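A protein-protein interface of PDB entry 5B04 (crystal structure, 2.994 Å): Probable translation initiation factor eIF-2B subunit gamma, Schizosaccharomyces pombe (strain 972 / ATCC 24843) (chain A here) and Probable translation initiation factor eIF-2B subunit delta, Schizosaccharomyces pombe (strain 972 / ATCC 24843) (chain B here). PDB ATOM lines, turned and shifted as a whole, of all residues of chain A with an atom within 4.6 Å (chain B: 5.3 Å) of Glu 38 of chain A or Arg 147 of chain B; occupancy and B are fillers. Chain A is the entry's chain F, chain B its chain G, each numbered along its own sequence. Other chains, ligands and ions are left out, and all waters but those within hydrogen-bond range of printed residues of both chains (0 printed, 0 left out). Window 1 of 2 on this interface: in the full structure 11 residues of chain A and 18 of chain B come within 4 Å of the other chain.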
ATOM      1  N   PRO A  36      -3.207  -0.918  20.013  1.00  0.00           N
ATOM      2  CA  PRO A  36      -3.603  -1.590  18.773  1.00  0.00           C
ATOM      3  C   PRO A  36      -2.437  -2.357  18.162  1.00  0.00           C
ATOM      4  O   PRO A  36      -1.316  -2.271  18.667  1.00  0.00           O
ATOM      5  CB  PRO A  36      -4.034  -0.431  17.871  1.00  0.00           C
ATOM      6  CG  PRO A  36      -3.232   0.725  18.357  1.00  0.00           C
ATOM      7  CD  PRO A  36      -3.114   0.543  19.845  1.00  0.00           C
ATOM      8  N   ILE A  37      -2.696  -3.098  17.092  1.00  0.00           N
ATOM      9  CA  ILE A  37      -1.644  -3.853  16.426  1.00  0.00           C
ATOM     10  C   ILE A  37      -0.917  -2.983  15.405  1.00  0.00           C
ATOM     11  O   ILE A  37      -1.531  -2.450  14.481  1.00  0.00           O
ATOM     12  CB  ILE A  37      -2.201  -5.106  15.728  1.00  0.00           C
ATOM     13  CG1 ILE A  37      -2.930  -5.995  16.737  1.00  0.00           C
ATOM     14  CG2 ILE A  37      -1.082  -5.878  15.048  1.00  0.00           C
ATOM     15  CD1 ILE A  37      -3.421  -7.304  16.159  1.00  0.00           C
ATOM     16  N   GLU A  38       0.393  -2.840  15.584  1.00  0.00           N
ATOM     17  CA  GLU A  38       1.208  -2.037  14.682  1.00  0.00           C
ATOM     18  C   GLU A  38       1.604  -2.844  13.450  1.00  0.00           C
ATOM     19  O   GLU A  38       1.442  -2.388  12.318  1.00  0.00           O
ATOM     20  CB  GLU A  38       2.455  -1.521  15.403  1.00  0.00           C
ATOM     21  CG  GLU A  38       3.250  -0.490  14.620  1.00  0.00           C
ATOM     22  CD  GLU A  38       4.462   0.012  15.380  1.00  0.00           C
ATOM     23  OE1 GLU A  38       4.727  -0.504  16.488  1.00  0.00           O
ATOM     24  OE2 GLU A  38       5.149   0.926  14.874  1.00  0.00           O
ATOM     25  N   PHE A  39       2.123  -4.047  13.680  1.00  0.00           N
ATOM     26  CA  PHE A  39       2.485  -4.944  12.588  1.00  0.00           C
ATOM     27  C   PHE A  39       1.932  -6.348  12.799  1.00  0.00           C
ATOM     28  O   PHE A  39       1.817  -6.820  13.931  1.00  0.00           O
ATOM     29  CB  PHE A  39       4.005  -5.028  12.426  1.00  0.00           C
ATOM     30  CG  PHE A  39       4.685  -3.698  12.285  1.00  0.00           C
ATOM     31  CD1 PHE A  39       4.479  -2.912  11.165  1.00  0.00           C
ATOM     32  CD2 PHE A  39       5.556  -3.247  13.264  1.00  0.00           C
ATOM     33  CE1 PHE A  39       5.113  -1.691  11.032  1.00  0.00           C
ATOM     34  CE2 PHE A  39       6.194  -2.029  13.136  1.00  0.00           C
ATOM     35  CZ  PHE A  39       5.972  -1.249  12.019  1.00  0.00           C
ATOM     36  N   GLN A  40       1.591  -7.011  11.700  1.00  0.00           N
ATOM     37  CA  GLN A  40       1.303  -8.438  11.722  1.00  0.00           C
ATOM     38  C   GLN A  40       2.294  -9.142  10.803  1.00  0.00           C
ATOM     39  O   GLN A  40       2.591  -8.655   9.713  1.00  0.00           O
ATOM     40  CB  GLN A  40      -0.142  -8.725  11.305  1.00  0.00           C
ATOM     41  CG  GLN A  40      -0.584  -8.040  10.023  1.00  0.00           C
ATOM     42  CD  GLN A  40      -2.054  -8.266   9.725  1.00  0.00           C
ATOM     43  OE1 GLN A  40      -2.628  -7.617   8.851  1.00  0.00           O
ATOM     44  NE2 GLN A  40      -2.670  -9.190  10.453  1.00  0.00           N
ATOM     45  N   ASN A 141      -3.191  -4.546   8.860  1.00  0.00           N
ATOM     46  CA  ASN A 141      -2.248  -3.516   9.282  1.00  0.00           C
ATOM     47  C   ASN A 141      -1.009  -3.502   8.398  1.00  0.00           C
ATOM     48  O   ASN A 141      -0.960  -4.193   7.380  1.00  0.00           O
ATOM     49  CB  ASN A 141      -1.839  -3.728  10.742  1.00  0.00           C
ATOM     50  CG  ASN A 141      -3.027  -3.931  11.660  1.00  0.00           C
ATOM     51  OD1 ASN A 141      -3.067  -4.881  12.442  1.00  0.00           O
ATOM     52  ND2 ASN A 141      -4.006  -3.039  11.567  1.00  0.00           N
ATOM     53  N   ASP A 142      -0.014  -2.707   8.781  1.00  0.00           N
ATOM     54  CA  ASP A 142       1.298  -2.788   8.152  1.00  0.00           C
ATOM     55  C   ASP A 142       1.850  -4.176   8.440  1.00  0.00           C
ATOM     56  O   ASP A 142       1.675  -4.694   9.542  1.00  0.00           O
ATOM     57  CB  ASP A 142       2.239  -1.700   8.674  1.00  0.00           C
ATOM     58  CG  ASP A 142       1.752  -0.301   8.351  1.00  0.00           C
ATOM     59  OD1 ASP A 142       1.057  -0.132   7.327  1.00  0.00           O
ATOM     60  OD2 ASP A 142       2.067   0.632   9.120  1.00  0.00           O
ATOM     61  N   PHE A 163      11.839   1.427   9.820  1.00  0.00           N
ATOM     62  CA  PHE A 163      10.568   1.538   9.115  1.00  0.00           C
ATOM     63  C   PHE A 163       9.664   2.560   9.795  1.00  0.00           C
ATOM     64  O   PHE A 163       8.876   3.241   9.139  1.00  0.00           O
ATOM     65  CB  PHE A 163       9.868   0.182   9.040  1.00  0.00           C
ATOM     66  CG  PHE A 163       8.563   0.218   8.298  1.00  0.00           C
ATOM     67  CD1 PHE A 163       8.535   0.454   6.933  1.00  0.00           C
ATOM     68  CD2 PHE A 163       7.365   0.018   8.962  1.00  0.00           C
ATOM     69  CE1 PHE A 163       7.338   0.491   6.246  1.00  0.00           C
ATOM     70  CE2 PHE A 163       6.164   0.052   8.280  1.00  0.00           C
ATOM     71  CZ  PHE A 163       6.151   0.289   6.919  1.00  0.00           C
ATOM     72  N   ARG A 164       9.785   2.662  11.114  1.00  0.00           N
ATOM     73  CA  ARG A 164       9.017   3.633  11.884  1.00  0.00           C
ATOM     74  C   ARG A 164       9.518   5.053  11.640  1.00  0.00           C
ATOM     75  O   ARG A 164       8.742   5.946  11.299  1.00  0.00           O
ATOM     76  CB  ARG A 164       9.085   3.306  13.377  1.00  0.00           C
ATOM     77  CG  ARG A 164       8.372   2.024  13.773  1.00  0.00           C
ATOM     78  CD  ARG A 164       8.876   1.507  15.110  1.00  0.00           C
ATOM     79  NE  ARG A 164       8.131   0.337  15.565  1.00  0.00           N
ATOM     80  CZ  ARG A 164       8.492  -0.425  16.593  1.00  0.00           C
ATOM     81  NH1 ARG A 164       9.595  -0.145  17.274  1.00  0.00           N
ATOM     82  NH2 ARG A 164       7.753  -1.470  16.937  1.00  0.00           N
ATOM     83  N   ASN A 167       9.497   6.001   7.845  1.00  0.00           N
ATOM     84  CA  ASN A 167       8.129   5.850   7.344  1.00  0.00           C
ATOM     85  C   ASN A 167       8.027   5.737   5.814  1.00  0.00           C
ATOM     86  O   ASN A 167       7.467   6.620   5.162  1.00  0.00           O
ATOM     87  CB  ASN A 167       7.269   7.017   7.837  1.00  0.00           C
ATOM     88  CG  ASN A 167       5.784   6.764   7.662  1.00  0.00           C
ATOM     89  OD1 ASN A 167       5.189   5.964   8.384  1.00  0.00           O
ATOM     90  ND2 ASN A 167       5.175   7.453   6.704  1.00  0.00           N
ATOM     91  N   PRO B 143       1.909   2.307  20.106  1.00  0.00           N
ATOM     92  CA  PRO B 143       2.678   2.472  18.866  1.00  0.00           C
ATOM     93  C   PRO B 143       2.984   3.929  18.520  1.00  0.00           C
ATOM     94  O   PRO B 143       4.130   4.251  18.207  1.00  0.00           O
ATOM     95  CB  PRO B 143       1.762   1.851  17.811  1.00  0.00           C
ATOM     96  CG  PRO B 143       1.034   0.791  18.551  1.00  0.00           C
ATOM     97  CD  PRO B 143       0.819   1.326  19.945  1.00  0.00           C
ATOM     98  N   ALA B 144       1.972   4.790  18.577  1.00  0.00           N
ATOM     99  CA  ALA B 144       2.148   6.206  18.268  1.00  0.00           C
ATOM    100  C   ALA B 144       3.143   6.861  19.220  1.00  0.00           C
ATOM    101  O   ALA B 144       3.853   7.794  18.845  1.00  0.00           O
ATOM    102  CB  ALA B 144       0.812   6.929  18.317  1.00  0.00           C
ATOM    103  N   VAL B 145       3.187   6.368  20.454  1.00  0.00           N
ATOM    104  CA  VAL B 145       4.141   6.858  21.441  1.00  0.00           C
ATOM    105  C   VAL B 145       5.556   6.418  21.074  1.00  0.00           C
ATOM    106  O   VAL B 145       6.513   7.179  21.225  1.00  0.00           O
ATOM    107  CB  VAL B 145       3.795   6.358  22.860  1.00  0.00           C
ATOM    108  CG1 VAL B 145       4.821   6.846  23.871  1.00  0.00           C
ATOM    109  CG2 VAL B 145       2.402   6.812  23.251  1.00  0.00           C
ATOM    110  N   ILE B 146       5.675   5.189  20.583  1.00  0.00           N
ATOM    111  CA  ILE B 146       6.967   4.628  20.198  1.00  0.00           C
ATOM    112  C   ILE B 146       7.619   5.425  19.071  1.00  0.00           C
ATOM    113  O   ILE B 146       8.786   5.807  19.166  1.00  0.00           O
ATOM    114  CB  ILE B 146       6.833   3.160  19.749  1.00  0.00           C
ATOM    115  CG1 ILE B 146       6.267   2.303  20.882  1.00  0.00           C
ATOM    116  CG2 ILE B 146       8.177   2.616  19.292  1.00  0.00           C
ATOM    117  CD1 ILE B 146       6.076   0.849  20.509  1.00  0.00           C
ATOM    118  N   ARG B 147       6.858   5.670  18.009  1.00  0.00           N
ATOM    119  CA  ARG B 147       7.361   6.405  16.854  1.00  0.00           C
ATOM    120  C   ARG B 147       7.736   7.832  17.233  1.00  0.00           C
ATOM    121  O   ARG B 147       8.673   8.407  16.678  1.00  0.00           O
ATOM    122  CB  ARG B 147       6.326   6.412  15.728  1.00  0.00           C
ATOM    123  CG  ARG B 147       5.730   5.047  15.432  1.00  0.00           C
ATOM    124  CD  ARG B 147       4.942   5.049  14.133  1.00  0.00           C
ATOM    125  NE  ARG B 147       4.424   3.723  13.812  1.00  0.00           N
ATOM    126  CZ  ARG B 147       4.547   3.139  12.624  1.00  0.00           C
ATOM    127  NH1 ARG B 147       5.178   3.763  11.638  1.00  0.00           N
ATOM    128  NH2 ARG B 147       4.043   1.929  12.422  1.00  0.00           N
ATOM    129  N   LEU B 148       6.999   8.398  18.183  1.00  0.00           N
ATOM    130  CA  LEU B 148       7.304   9.728  18.693  1.00  0.00           C
ATOM    131  C   LEU B 148       8.609   9.696  19.478  1.00  0.00           C
ATOM    132  O   LEU B 148       9.400  10.636  19.425  1.00  0.00           O
ATOM    133  CB  LEU B 148       6.167  10.248  19.572  1.00  0.00           C
ATOM    134  CG  LEU B 148       6.283  11.703  20.030  1.00  0.00           C
ATOM    135  CD1 LEU B 148       6.127  12.649  18.848  1.00  0.00           C
ATOM    136  CD2 LEU B 148       5.261  12.013  21.113  1.00  0.00           C
ATOM    137  N   GLY B 149       8.826   8.603  20.203  1.00  0.00           N
ATOM    138  CA  GLY B 149      10.045   8.422  20.970  1.00  0.00           C
ATOM    139  C   GLY B 149      11.265   8.334  20.076  1.00  0.00           C
ATOM    140  O   GLY B 149      12.334   8.837  20.419  1.00  0.00           O
ATOM    141  N   LEU B 150      11.102   7.690  18.925  1.00  0.00           N
ATOM    142  CA  LEU B 150      12.185   7.577  17.957  1.00  0.00           C
ATOM    143  C   LEU B 150      12.507   8.930  17.331  1.00  0.00           C
ATOM    144  O   LEU B 150      13.670   9.311  17.225  1.00  0.00           O
ATOM    145  CB  LEU B 150      11.831   6.567  16.863  1.00  0.00           C
ATOM    146  CG  LEU B 150      11.685   5.106  17.286  1.00  0.00           C
ATOM    147  CD1 LEU B 150      11.379   4.237  16.078  1.00  0.00           C
ATOM    148  CD2 LEU B 150      12.940   4.620  17.994  1.00  0.00           C
ATOM    149  N   LYS B 151      11.469   9.655  16.926  1.00  0.00           N
ATOM    150  CA  LYS B 151      11.648  10.929  16.240  1.00  0.00           C
ATOM    151  C   LYS B 151      12.182  12.011  17.173  1.00  0.00           C
ATOM    152  O   LYS B 151      12.951  12.877  16.753  1.00  0.00           O
ATOM    153  CB  LYS B 151      10.333  11.385  15.610  1.00  0.00           C
ATOM    154  CG  LYS B 151      10.403  11.500  14.100  1.00  0.00           C
ATOM    155  CD  LYS B 151       9.227  12.274  13.533  1.00  0.00           C
ATOM    156  CE  LYS B 151       7.913  11.859  14.163  1.00  0.00           C
ATOM    157  NZ  LYS B 151       6.777  12.571  13.518  1.00  0.00           N
ATOM    158  N   LEU B 152      11.770  11.962  18.434  1.00  0.00           N
ATOM    159  CA  LEU B 152      12.293  12.883  19.435  1.00  0.00           C
ATOM    160  C   LEU B 152      13.785  12.658  19.632  1.00  0.00           C
ATOM    161  O   LEU B 152      14.560  13.608  19.743  1.00  0.00           O
ATOM    162  CB  LEU B 152      11.560  12.720  20.769  1.00  0.00           C
ATOM    163  CG  LEU B 152      10.183  13.369  20.911  1.00  0.00           C
ATOM    164  CD1 LEU B 152       9.542  12.965  22.229  1.00  0.00           C
ATOM    165  CD2 LEU B 152      10.298  14.882  20.808  1.00  0.00           C
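The side-chain carboxylate of Glu 38 of chain A lies within salt-bridge range of the guanidinium group of Arg 147 of chain B (2.9 Å).
Printed residues of chain B within 4 Å of Pro 36 of chain A: Pro 143. Of the printed residues of chain B, Glu 38 of chain A touches Arg 147 (2.9 Å). Phe 163 of chain A touches none of the printed residues of chain B. Of the printed residues of chain A, Ile 146 of chain B touches Arg 164 (3.7 Å). Arg 147 of chain B touches just these residues of chain A: Glu 38 (2.9 Å), Phe 39 (3.7 Å), Arg 164 (3.8 Å) and Asn 167 (3.9 Å). Leu 152 of chain B touches none of the printed residues of chain A. The nearest printed residue of chain A that does not touch Leu 150 of chain B is Phe 163 of chain A (6.7 Å).
OE2 of Glu 38 of chain A is in salt-bridge range of NE of Arg 164 of chain A, 3.1 Å away.
Among the printed residues, merely in contact across the chains: Arg 164 of chain A with Leu 150 of chain B (3.7 Å), Arg 164 of chain A with Ile 146 of chain B (3.7 Å), Phe 39 of chain A with Arg 147 of chain B (3.7 Å), Arg 164 of chain A with Arg 147 of chain B (3.8 Å), Pro 36 of chain A with Pro 143 of chain B (3.9 Å) and Asn 167 of chain A with Arg 147 of chain B (3.9 Å).
Of the 10 printed residues of chain B, 4 touch a printed residue of chain A. Of the 10 printed residues of chain A, 5 touch a printed residue of chain B. Printed residues of chain A that touch a printed residue of chain B: Pro 36, Glu 38, Phe 39, Arg 164 and Asn 167.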
